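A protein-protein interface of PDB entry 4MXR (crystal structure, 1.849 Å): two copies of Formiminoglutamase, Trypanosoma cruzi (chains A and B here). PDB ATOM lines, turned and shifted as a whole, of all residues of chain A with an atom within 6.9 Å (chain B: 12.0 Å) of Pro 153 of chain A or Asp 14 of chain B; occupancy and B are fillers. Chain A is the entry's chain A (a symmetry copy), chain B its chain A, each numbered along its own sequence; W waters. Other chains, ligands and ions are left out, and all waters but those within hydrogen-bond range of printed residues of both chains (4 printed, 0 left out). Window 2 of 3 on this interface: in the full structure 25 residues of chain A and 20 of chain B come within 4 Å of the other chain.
A ring nitrogen (NE2) of His 194 of chain A lies within hydrogen-bond range of the side-chain carboxylate of Asp 14 of chain B, at 2.8 Å.
The side-chain carboxylate of Asp 15 of chain B lies within salt-bridge range of the guanidinium group of Arg 152 of chain A, 3.8 Å away.
NH2 of Arg 17 of chain B lies within salt-bridge range of OD2 of Asp 15 of chain B (3.6 Å).
The side-chain hydroxyl (OG) of Ser 20 of chain B is in hydrogen-bond range of the backbone carbonyl oxygen (O) of Arg 17 of chain B, at 2.6 Å.
O of Arg 65 of chain B sits at hydrogen-bond distance from NH1 of Arg 17 of chain B, at 2.9 Å.
N of Arg 152 of chain A sits at hydrogen-bond distance from O of Gly 163 of chain A, 2.9 Å away.
O of Pro 153 of chain A sits at hydrogen-bond distance from NE2 of His 161 of chain A (2.9 Å).
NH2 of Arg 17 of chain B touches NH2 of Arg 152 of chain A (3.9 Å).
Pro 153 of chain A touches Asp 14 of chain B (CD to OD2, 3.4 Å).
Asp 15 of chain B touches Gly 191 of chain A.
Ala 192 of chain A touches Asn 70 of chain B.
CB of Ala 192 of chain A touches CD1 of Leu 72 of chain B (3.5 Å).
Leu 193 of chain A touches Asp 14 of chain B (CD1 to O, 3.5 Å).
Of chain B, only Asp 14 comes within 4 Å of Pro 153 of chain A.
Of chain A, only Pro 153, Leu 193 and His 194 come within 4 Å of Asp 14 of chain B.
Of chain B, only Asp 15 (3.8 Å) and Arg 17 (3.9 Å) come within 4 Å of Arg 152 of chain A.
No residue of chain B comes within 4 Å of Leu 155 of chain A.
No residue of chain B comes within 4 Å of Gly 163 of chain A.
No residue of chain B comes within 4 Å of Thr 164 of chain A.
Gly 191 of chain A touches just one residue of chain B: Asp 15 (3.4 Å).
Of chain B, only Asn 70 (3.6 Å) and Leu 72 (3.5 Å) come within 4 Å of Ala 192 of chain A.
Of chain B, only Asp 14 comes within 4 Å of Leu 193 of chain A.
Of the printed residues of chain B, His 194 of chain A touches Asp 14 (2.8 Å).
Printed residues of chain A within 4 Å of Asp 15 of chain B: Arg 152 (3.8 Å) and Gly 191 (3.4 Å).
Of the printed residues of chain A, Arg 17 of chain B touches Arg 152.
Printed residues of chain A within 4 Å of Leu 72 of chain B: Ala 192.
Of the 16 printed residues of chain B, 5 touch a printed residue of chain A.
Hydrophobic or aromatic side chains of chain B that line the printed part of chain A: Leu 72.
Hydrophobic or aromatic side chains of chain A that line the printed part of chain B: Pro 153, Ala 192, Leu 193 and His 194.
No position is printed for both chains.
Of the 8 pairs that touch across the chains among the printed residues, none has its exchanged pair printed and touching as well.
Water W4 lies within hydrogen-bond range of O of Asp 14 of chain B (2.8 Å), N of His 194 of chain A (3.2 Å), N of Leu 193 of chain A (3.4 Å) and O of Gly 191 of chain A (3.5 Å).
Water W2 lies within hydrogen-bond range of a ring nitrogen (ND1) of His 194 of chain A (2.8 Å), the backbone NH (N) of Gly 191 of chain A (3.0 Å) and the side-chain carboxylate (OD2) of Asp 15 of chain B (3.1 Å).
Water W1 lies within hydrogen-bond range of the backbone NH of Leu 193 of chain A, the backbone NH of Ala 192 of chain A and the backbone carbonyl oxygen of Asp 14 of chain B.
Water W3 lies within hydrogen-bond range of N of Ala 192 of chain A and O of Asn 70 of chain B.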
ATOM      1  N   ASN A  46      17.140   3.355   9.141  1.00  0.00           N
ATOM      2  CA  ASN A  46      17.300   3.715  10.547  1.00  0.00           C
ATOM      3  C   ASN A  46      15.989   3.520  11.309  1.00  0.00           C
ATOM      4  O   ASN A  46      15.862   3.922  12.467  1.00  0.00           O
ATOM      5  CB  ASN A  46      17.770   5.171  10.659  1.00  0.00           C
ATOM      6  CG  ASN A  46      18.350   5.506  12.024  1.00  0.00           C
ATOM      7  OD1 ASN A  46      18.766   4.623  12.776  1.00  0.00           O
ATOM      8  ND2 ASN A  46      18.388   6.794  12.345  1.00  0.00           N
ATOM      9  N   VAL A 151      25.435   8.482  15.846  1.00  0.00           N
ATOM     10  CA  VAL A 151      26.686   7.738  15.794  1.00  0.00           C
ATOM     11  C   VAL A 151      26.382   6.249  15.926  1.00  0.00           C
ATOM     12  O   VAL A 151      27.192   5.475  16.438  1.00  0.00           O
ATOM     13  CB  VAL A 151      27.689   8.199  16.878  1.00  0.00           C
ATOM     14  CG1 VAL A 151      28.216   9.592  16.557  1.00  0.00           C
ATOM     15  CG2 VAL A 151      27.046   8.177  18.255  1.00  0.00           C
ATOM     16  N   ARG A 152      25.198   5.863  15.458  1.00  0.00           N
ATOM     17  CA  ARG A 152      24.792   4.466  15.425  1.00  0.00           C
ATOM     18  C   ARG A 152      25.676   3.672  14.471  1.00  0.00           C
ATOM     19  O   ARG A 152      26.192   4.217  13.491  1.00  0.00           O
ATOM     20  CB  ARG A 152      23.327   4.338  14.991  1.00  0.00           C
ATOM     21  CG  ARG A 152      22.352   5.091  15.875  1.00  0.00           C
ATOM     22  CD  ARG A 152      20.916   4.669  15.612  1.00  0.00           C
ATOM     23  NE  ARG A 152      19.980   5.460  16.406  1.00  0.00           N
ATOM     24  CZ  ARG A 152      19.705   5.231  17.688  1.00  0.00           C
ATOM     25  NH1 ARG A 152      20.291   4.228  18.332  1.00  0.00           N
ATOM     26  NH2 ARG A 152      18.842   6.010  18.326  1.00  0.00           N
ATOM     27  N   PRO A 153      25.858   2.375  14.758  1.00  0.00           N
ATOM     28  CA  PRO A 153      26.572   1.471  13.850  1.00  0.00           C
ATOM     29  C   PRO A 153      25.806   1.310  12.543  1.00  0.00           C
ATOM     30  O   PRO A 153      24.606   1.592  12.498  1.00  0.00           O
ATOM     31  CB  PRO A 153      26.566   0.133  14.603  1.00  0.00           C
ATOM     32  CG  PRO A 153      26.256   0.470  16.023  1.00  0.00           C
ATOM     33  CD  PRO A 153      25.396   1.692  15.979  1.00  0.00           C
ATOM     34  N   PRO A 154      26.487   0.851  11.484  1.00  0.00           N
ATOM     35  CA  PRO A 154      25.803   0.529  10.226  1.00  0.00           C
ATOM     36  C   PRO A 154      24.875  -0.661  10.446  1.00  0.00           C
ATOM     37  O   PRO A 154      24.877  -1.237  11.534  1.00  0.00           O
ATOM     38  CB  PRO A 154      26.950   0.110   9.298  1.00  0.00           C
ATOM     39  CG  PRO A 154      28.208   0.588   9.963  1.00  0.00           C
ATOM     40  CD  PRO A 154      27.929   0.561  11.425  1.00  0.00           C
ATOM     41  N   LEU A 155      24.095  -1.025   9.435  1.00  0.00           N
ATOM     42  CA  LEU A 155      23.309  -2.248   9.516  1.00  0.00           C
ATOM     43  C   LEU A 155      24.250  -3.446   9.449  1.00  0.00           C
ATOM     44  O   LEU A 155      25.379  -3.331   8.966  1.00  0.00           O
ATOM     45  CB  LEU A 155      22.272  -2.315   8.394  1.00  0.00           C
ATOM     46  CG  LEU A 155      21.238  -1.188   8.328  1.00  0.00           C
ATOM     47  CD1 LEU A 155      20.166  -1.519   7.298  1.00  0.00           C
ATOM     48  CD2 LEU A 155      20.608  -0.948   9.691  1.00  0.00           C
ATOM     49  N   SER A 156      23.782  -4.591   9.932  1.00  0.00           N
ATOM     50  CA  SER A 156      24.611  -5.791  10.025  1.00  0.00           C
ATOM     51  C   SER A 156      25.254  -6.198   8.697  1.00  0.00           C
ATOM     52  O   SER A 156      26.255  -6.917   8.682  1.00  0.00           O
ATOM     53  CB  SER A 156      23.801  -6.959  10.598  1.00  0.00           C
ATOM     54  OG  SER A 156      22.696  -7.266   9.766  1.00  0.00           O
ATOM     55  N   ARG A 159      25.412  -1.653   5.604  1.00  0.00           N
ATOM     56  CA  ARG A 159      24.709  -0.509   5.025  1.00  0.00           C
ATOM     57  C   ARG A 159      24.641   0.701   5.960  1.00  0.00           C
ATOM     58  O   ARG A 159      24.416   0.560   7.162  1.00  0.00           O
ATOM     59  CB  ARG A 159      23.302  -0.912   4.583  1.00  0.00           C
ATOM     60  CG  ARG A 159      23.266  -1.823   3.364  1.00  0.00           C
ATOM     61  CD  ARG A 159      21.835  -2.142   2.967  1.00  0.00           C
ATOM     62  NE  ARG A 159      21.110  -2.795   4.052  1.00  0.00           N
ATOM     63  CZ  ARG A 159      19.797  -3.000   4.060  1.00  0.00           C
ATOM     64  NH1 ARG A 159      19.054  -2.599   3.037  1.00  0.00           N
ATOM     65  NH2 ARG A 159      19.225  -3.605   5.092  1.00  0.00           N
ATOM     66  N   VAL A 160      24.829   1.889   5.390  1.00  0.00           N
ATOM     67  CA  VAL A 160      24.763   3.131   6.155  1.00  0.00           C
ATOM     68  C   VAL A 160      23.332   3.662   6.202  1.00  0.00           C
ATOM     69  O   VAL A 160      22.512   3.333   5.347  1.00  0.00           O
ATOM     70  CB  VAL A 160      25.686   4.213   5.553  1.00  0.00           C
ATOM     71  CG1 VAL A 160      27.129   3.722   5.522  1.00  0.00           C
ATOM     72  CG2 VAL A 160      25.212   4.598   4.156  1.00  0.00           C
ATOM     73  N   HIS A 161      23.028   4.474   7.209  1.00  0.00           N
ATOM     74  CA  HIS A 161      21.691   5.049   7.334  1.00  0.00           C
ATOM     75  C   HIS A 161      21.701   6.442   7.967  1.00  0.00           C
ATOM     76  O   HIS A 161      22.760   6.975   8.302  1.00  0.00           O
ATOM     77  CB  HIS A 161      20.754   4.106   8.097  1.00  0.00           C
ATOM     78  CG  HIS A 161      21.296   3.630   9.411  1.00  0.00           C
ATOM     79  ND1 HIS A 161      21.182   4.361  10.574  1.00  0.00           N
ATOM     80  CD2 HIS A 161      21.938   2.486   9.749  1.00  0.00           C
ATOM     81  CE1 HIS A 161      21.734   3.691  11.570  1.00  0.00           C
ATOM     82  NE2 HIS A 161      22.201   2.551  11.097  1.00  0.00           N
ATOM     83  N   GLY A 163      21.248   7.372  10.705  1.00  0.00           N
ATOM     84  CA  GLY A 163      21.741   7.377  12.072  1.00  0.00           C
ATOM     85  C   GLY A 163      23.237   7.163  12.240  1.00  0.00           C
ATOM     86  O   GLY A 163      23.742   7.135  13.362  1.00  0.00           O
ATOM     87  N   THR A 164      23.956   7.016  11.132  1.00  0.00           N
ATOM     88  CA  THR A 164      25.384   6.718  11.203  1.00  0.00           C
ATOM     89  C   THR A 164      26.333   7.823  10.726  1.00  0.00           C
ATOM     90  O   THR A 164      27.545   7.653  10.816  1.00  0.00           O
ATOM     91  CB  THR A 164      25.732   5.457  10.387  1.00  0.00           C
ATOM     92  OG1 THR A 164      25.618   5.744   8.988  1.00  0.00           O
ATOM     93  CG2 THR A 164      24.810   4.306  10.751  1.00  0.00           C
ATOM     94  N   ARG A 167      29.247   8.866  13.101  1.00  0.00           N
ATOM     95  CA  ARG A 167      30.162   7.763  13.364  1.00  0.00           C
ATOM     96  C   ARG A 167      31.136   7.669  12.188  1.00  0.00           C
ATOM     97  O   ARG A 167      32.341   7.504  12.373  1.00  0.00           O
ATOM     98  CB  ARG A 167      29.398   6.447  13.535  1.00  0.00           C
ATOM     99  CG  ARG A 167      30.253   5.289  14.036  1.00  0.00           C
ATOM    100  CD  ARG A 167      29.392   4.149  14.577  1.00  0.00           C
ATOM    101  NE  ARG A 167      30.155   3.238  15.427  1.00  0.00           N
ATOM    102  CZ  ARG A 167      29.789   2.867  16.649  1.00  0.00           C
ATOM    103  NH1 ARG A 167      28.663   3.325  17.180  1.00  0.00           N
ATOM    104  NH2 ARG A 167      30.550   2.034  17.347  1.00  0.00           N
ATOM    105  N   GLY A 191      21.801   7.326  23.857  1.00  0.00           N
ATOM    106  CA  GLY A 191      22.265   6.240  24.703  1.00  0.00           C
ATOM    107  C   GLY A 191      23.610   6.484  25.369  1.00  0.00           C
ATOM    108  O   GLY A 191      24.441   7.242  24.864  1.00  0.00           O
ATOM    109  N   ALA A 192      23.823   5.837  26.511  1.00  0.00           N
ATOM    110  CA  ALA A 192      25.078   5.963  27.243  1.00  0.00           C
ATOM    111  C   ALA A 192      26.275   5.517  26.401  1.00  0.00           C
ATOM    112  O   ALA A 192      27.338   6.138  26.444  1.00  0.00           O
ATOM    113  CB  ALA A 192      25.016   5.178  28.539  1.00  0.00           C
ATOM    114  N   LEU A 193      26.096   4.442  25.637  1.00  0.00           N
ATOM    115  CA  LEU A 193      27.155   3.936  24.764  1.00  0.00           C
ATOM    116  C   LEU A 193      27.544   4.941  23.683  1.00  0.00           C
ATOM    117  O   LEU A 193      28.725   5.117  23.380  1.00  0.00           O
ATOM    118  CB  LEU A 193      26.734   2.622  24.101  1.00  0.00           C
ATOM    119  CG  LEU A 193      26.751   1.343  24.939  1.00  0.00           C
ATOM    120  CD1 LEU A 193      26.290   0.164  24.092  1.00  0.00           C
ATOM    121  CD2 LEU A 193      28.137   1.087  25.509  1.00  0.00           C
ATOM    122  N   HIS A 194      26.550   5.589  23.087  1.00  0.00           N
ATOM    123  CA  HIS A 194      26.824   6.534  22.012  1.00  0.00           C
ATOM    124  C   HIS A 194      27.432   7.831  22.541  1.00  0.00           C
ATOM    125  O   HIS A 194      28.288   8.424  21.891  1.00  0.00           O
ATOM    126  CB  HIS A 194      25.571   6.785  21.176  1.00  0.00           C
ATOM    127  CG  HIS A 194      25.062   5.557  20.490  1.00  0.00           C
ATOM    128  ND1 HIS A 194      23.813   5.488  19.908  1.00  0.00           N
ATOM    129  CD2 HIS A 194      25.630   4.342  20.302  1.00  0.00           C
ATOM    130  CE1 HIS A 194      23.639   4.289  19.386  1.00  0.00           C
ATOM    131  NE2 HIS A 194      24.727   3.572  19.612  1.00  0.00           N
ATOM    132  N   ASP B  14      22.086  -1.593  21.460  1.00  0.00           N
ATOM    133  CA  ASP B  14      23.136  -0.803  22.094  1.00  0.00           C
ATOM    134  C   ASP B  14      22.593   0.504  22.678  1.00  0.00           C
ATOM    135  O   ASP B  14      23.328   1.479  22.844  1.00  0.00           O
ATOM    136  CB  ASP B  14      24.270  -0.516  21.102  1.00  0.00           C
ATOM    137  CG  ASP B  14      23.807   0.281  19.893  1.00  0.00           C
ATOM    138  OD1 ASP B  14      22.579   0.396  19.680  1.00  0.00           O
ATOM    139  OD2 ASP B  14      24.676   0.790  19.151  1.00  0.00           O
ATOM    140  N   ASP B  15      21.303   0.513  22.995  1.00  0.00           N
ATOM    141  CA  ASP B  15      20.651   1.699  23.536  1.00  0.00           C
ATOM    142  C   ASP B  15      19.408   1.297  24.327  1.00  0.00           C
ATOM    143  O   ASP B  15      18.282   1.532  23.886  1.00  0.00           O
ATOM    144  CB  ASP B  15      20.278   2.652  22.397  1.00  0.00           C
ATOM    145  CG  ASP B  15      19.766   3.997  22.892  1.00  0.00           C
ATOM    146  OD1 ASP B  15      19.592   4.172  24.119  1.00  0.00           O
ATOM    147  OD2 ASP B  15      19.534   4.882  22.040  1.00  0.00           O
ATOM    148  N   PRO B  16      19.613   0.682  25.502  1.00  0.00           N
ATOM    149  CA  PRO B  16      18.505   0.205  26.335  1.00  0.00           C
ATOM    150  C   PRO B  16      17.537   1.329  26.667  1.00  0.00           C
ATOM    151  O   PRO B  16      17.967   2.405  27.086  1.00  0.00           O
ATOM    152  CB  PRO B  16      19.204  -0.263  27.615  1.00  0.00           C
ATOM    153  CG  PRO B  16      20.600  -0.554  27.209  1.00  0.00           C
ATOM    154  CD  PRO B  16      20.922   0.438  26.131  1.00  0.00           C
ATOM    155  N   ARG B  17      16.245   1.077  26.487  1.00  0.00           N
ATOM    156  CA  ARG B  17      15.227   2.064  26.821  1.00  0.00           C
ATOM    157  C   ARG B  17      14.195   1.508  27.801  1.00  0.00           C
ATOM    158  O   ARG B  17      14.409   0.461  28.403  1.00  0.00           O
ATOM    159  CB  ARG B  17      14.576   2.615  25.550  1.00  0.00           C
ATOM    160  CG  ARG B  17      15.530   3.501  24.759  1.00  0.00           C
ATOM    161  CD  ARG B  17      14.929   4.047  23.475  1.00  0.00           C
ATOM    162  NE  ARG B  17      15.816   5.043  22.876  1.00  0.00           N
ATOM    163  CZ  ARG B  17      15.555   5.716  21.760  1.00  0.00           C
ATOM    164  NH1 ARG B  17      14.422   5.504  21.101  1.00  0.00           N
ATOM    165  NH2 ARG B  17      16.428   6.605  21.302  1.00  0.00           N
ATOM    166  N   LEU B  18      13.086   2.218  27.974  1.00  0.00           N
ATOM    167  CA  LEU B  18      12.091   1.831  28.972  1.00  0.00           C
ATOM    168  C   LEU B  18      11.711   0.350  28.916  1.00  0.00           C
ATOM    169  O   LEU B  18      11.637  -0.317  29.948  1.00  0.00           O
ATOM    170  CB  LEU B  18      10.840   2.707  28.866  1.00  0.00           C
ATOM    171  CG  LEU B  18      10.948   4.058  29.576  1.00  0.00           C
ATOM    172  CD1 LEU B  18       9.690   4.877  29.381  1.00  0.00           C
ATOM    173  CD2 LEU B  18      11.225   3.859  31.060  1.00  0.00           C
ATOM    174  N   LEU B  19      11.473  -0.156  27.711  1.00  0.00           N
ATOM    175  CA  LEU B  19      11.084  -1.549  27.525  1.00  0.00           C
ATOM    176  C   LEU B  19      12.055  -2.504  28.217  1.00  0.00           C
ATOM    177  O   LEU B  19      11.651  -3.538  28.746  1.00  0.00           O
ATOM    178  CB  LEU B  19      10.989  -1.881  26.034  1.00  0.00           C
ATOM    179  CG  LEU B  19      10.607  -3.312  25.647  1.00  0.00           C
ATOM    180  CD1 LEU B  19       9.243  -3.687  26.219  1.00  0.00           C
ATOM    181  CD2 LEU B  19      10.622  -3.477  24.138  1.00  0.00           C
ATOM    182  N   SER B  20      13.334  -2.146  28.221  1.00  0.00           N
ATOM    183  CA  SER B  20      14.370  -3.005  28.792  1.00  0.00           C
ATOM    184  C   SER B  20      14.195  -3.188  30.297  1.00  0.00           C
ATOM    185  O   SER B  20      14.774  -4.099  30.887  1.00  0.00           O
ATOM    186  CB  SER B  20      15.762  -2.440  28.497  1.00  0.00           C
ATOM    187  OG  SER B  20      16.049  -1.334  29.340  1.00  0.00           O
ATOM    188  N   ARG B  65       9.132   1.976  22.741  1.00  0.00           N
ATOM    189  CA  ARG B  65      10.085   2.606  21.832  1.00  0.00           C
ATOM    190  C   ARG B  65      10.943   3.713  22.439  1.00  0.00           C
ATOM    191  O   ARG B  65      12.006   4.027  21.913  1.00  0.00           O
ATOM    192  CB  ARG B  65       9.344   3.151  20.605  1.00  0.00           C
ATOM    193  CG  ARG B  65       8.786   2.067  19.697  1.00  0.00           C
ATOM    194  CD  ARG B  65       7.693   2.592  18.777  1.00  0.00           C
ATOM    195  NE  ARG B  65       7.269   1.573  17.819  1.00  0.00           N
ATOM    196  CZ  ARG B  65       6.404   0.598  18.088  1.00  0.00           C
ATOM    197  NH1 ARG B  65       5.858   0.499  19.293  1.00  0.00           N
ATOM    198  NH2 ARG B  65       6.084  -0.286  17.151  1.00  0.00           N
ATOM    199  N   GLY B  67      12.729   6.391  25.600  1.00  0.00           N
ATOM    200  CA  GLY B  67      13.258   6.642  26.929  1.00  0.00           C
ATOM    201  C   GLY B  67      14.534   5.917  27.305  1.00  0.00           C
ATOM    202  O   GLY B  67      14.480   4.826  27.866  1.00  0.00           O
ATOM    203  N   SER B  68      15.677   6.534  27.012  1.00  0.00           N
ATOM    204  CA  SER B  68      16.981   5.993  27.389  1.00  0.00           C
ATOM    205  C   SER B  68      17.046   5.714  28.890  1.00  0.00           C
ATOM    206  O   SER B  68      16.885   6.623  29.705  1.00  0.00           O
ATOM    207  CB  SER B  68      18.100   6.964  26.998  1.00  0.00           C
ATOM    208  OG  SER B  68      18.084   7.250  25.608  1.00  0.00           O
ATOM    209  N   VAL B  69      17.300   4.459  29.254  1.00  0.00           N
ATOM    210  CA  VAL B  69      17.326   4.069  30.663  1.00  0.00           C
ATOM    211  C   VAL B  69      18.433   4.779  31.434  1.00  0.00           C
ATOM    212  O   VAL B  69      18.276   5.093  32.617  1.00  0.00           O
ATOM    213  CB  VAL B  69      17.482   2.546  30.839  1.00  0.00           C
ATOM    214  CG1 VAL B  69      16.267   1.830  30.286  1.00  0.00           C
ATOM    215  CG2 VAL B  69      18.750   2.061  30.164  1.00  0.00           C
ATOM    216  N   ASN B  70      19.554   5.024  30.765  1.00  0.00           N
ATOM    217  CA  ASN B  70      20.628   5.792  31.374  1.00  0.00           C
ATOM    218  C   ASN B  70      20.729   7.150  30.704  1.00  0.00           C
ATOM    219  O   ASN B  70      21.202   7.260  29.570  1.00  0.00           O
ATOM    220  CB  ASN B  70      21.958   5.042  31.284  1.00  0.00           C
ATOM    221  CG  ASN B  70      23.050   5.693  32.108  1.00  0.00           C
ATOM    222  OD1 ASN B  70      22.818   6.684  32.806  1.00  0.00           O
ATOM    223  ND2 ASN B  70      24.251   5.141  32.029  1.00  0.00           N
ATOM    224  N   ASN B  71      20.270   8.178  31.411  1.00  0.00           N
ATOM    225  CA  ASN B  71      20.160   9.522  30.862  1.00  0.00           C
ATOM    226  C   ASN B  71      21.343  10.398  31.268  1.00  0.00           C
ATOM    227  O   ASN B  71      21.416  10.882  32.399  1.00  0.00           O
ATOM    228  CB  ASN B  71      18.836  10.158  31.307  1.00  0.00           C
ATOM    229  CG  ASN B  71      18.595  11.520  30.674  1.00  0.00           C
ATOM    230  OD1 ASN B  71      19.505  12.340  30.569  1.00  0.00           O
ATOM    231  ND2 ASN B  71      17.355  11.770  30.261  1.00  0.00           N
ATOM    232  N   LEU B  72      22.270  10.604  30.340  1.00  0.00           N
ATOM    233  CA  LEU B  72      23.493  11.337  30.651  1.00  0.00           C
ATOM    234  C   LEU B  72      23.312  12.853  30.696  1.00  0.00           C
ATOM    235  O   LEU B  72      24.206  13.573  31.138  1.00  0.00           O
ATOM    236  CB  LEU B  72      24.632  10.940  29.703  1.00  0.00           C
ATOM    237  CG  LEU B  72      25.372   9.667  30.131  1.00  0.00           C
ATOM    238  CD1 LEU B  72      24.532   8.426  29.869  1.00  0.00           C
ATOM    239  CD2 LEU B  72      26.719   9.552  29.438  1.00  0.00           C
ATOM    240  N   ASP B  77      20.719   7.054  36.111  1.00  0.00           N
ATOM    241  CA  ASP B  77      20.645   5.710  35.564  1.00  0.00           C
ATOM    242  C   ASP B  77      19.495   4.965  36.237  1.00  0.00           C
ATOM    243  O   ASP B  77      19.501   4.768  37.451  1.00  0.00           O
ATOM    244  CB  ASP B  77      21.968   4.971  35.787  1.00  0.00           C
ATOM    245  CG  ASP B  77      21.944   3.555  35.246  1.00  0.00           C
ATOM    246  OD1 ASP B  77      21.146   3.285  34.324  1.00  0.00           O
ATOM    247  OD2 ASP B  77      22.723   2.713  35.745  1.00  0.00           O
ATOM    248  N   SER B  79      18.610   1.912  35.318  1.00  0.00           N
ATOM    249  CA  SER B  79      18.828   0.515  34.941  1.00  0.00           C
ATOM    250  C   SER B  79      18.392  -0.496  35.999  1.00  0.00           C
ATOM    251  O   SER B  79      18.113  -1.652  35.681  1.00  0.00           O
ATOM    252  CB  SER B  79      20.307   0.276  34.616  1.00  0.00           C
ATOM    253  OG  SER B  79      20.672   0.883  33.394  1.00  0.00           O
HETATM  254  O   HOH W   1      23.801   2.701  25.901  1.00  0.00           O
HETATM  255  O   HOH W   2      21.595   6.961  20.911  1.00  0.00           O
HETATM  256  O   HOH W   3      21.317   4.478  27.762  1.00  0.00           O
HETATM  257  O   HOH W   4      23.641   4.207  23.351  1.00  0.00           O
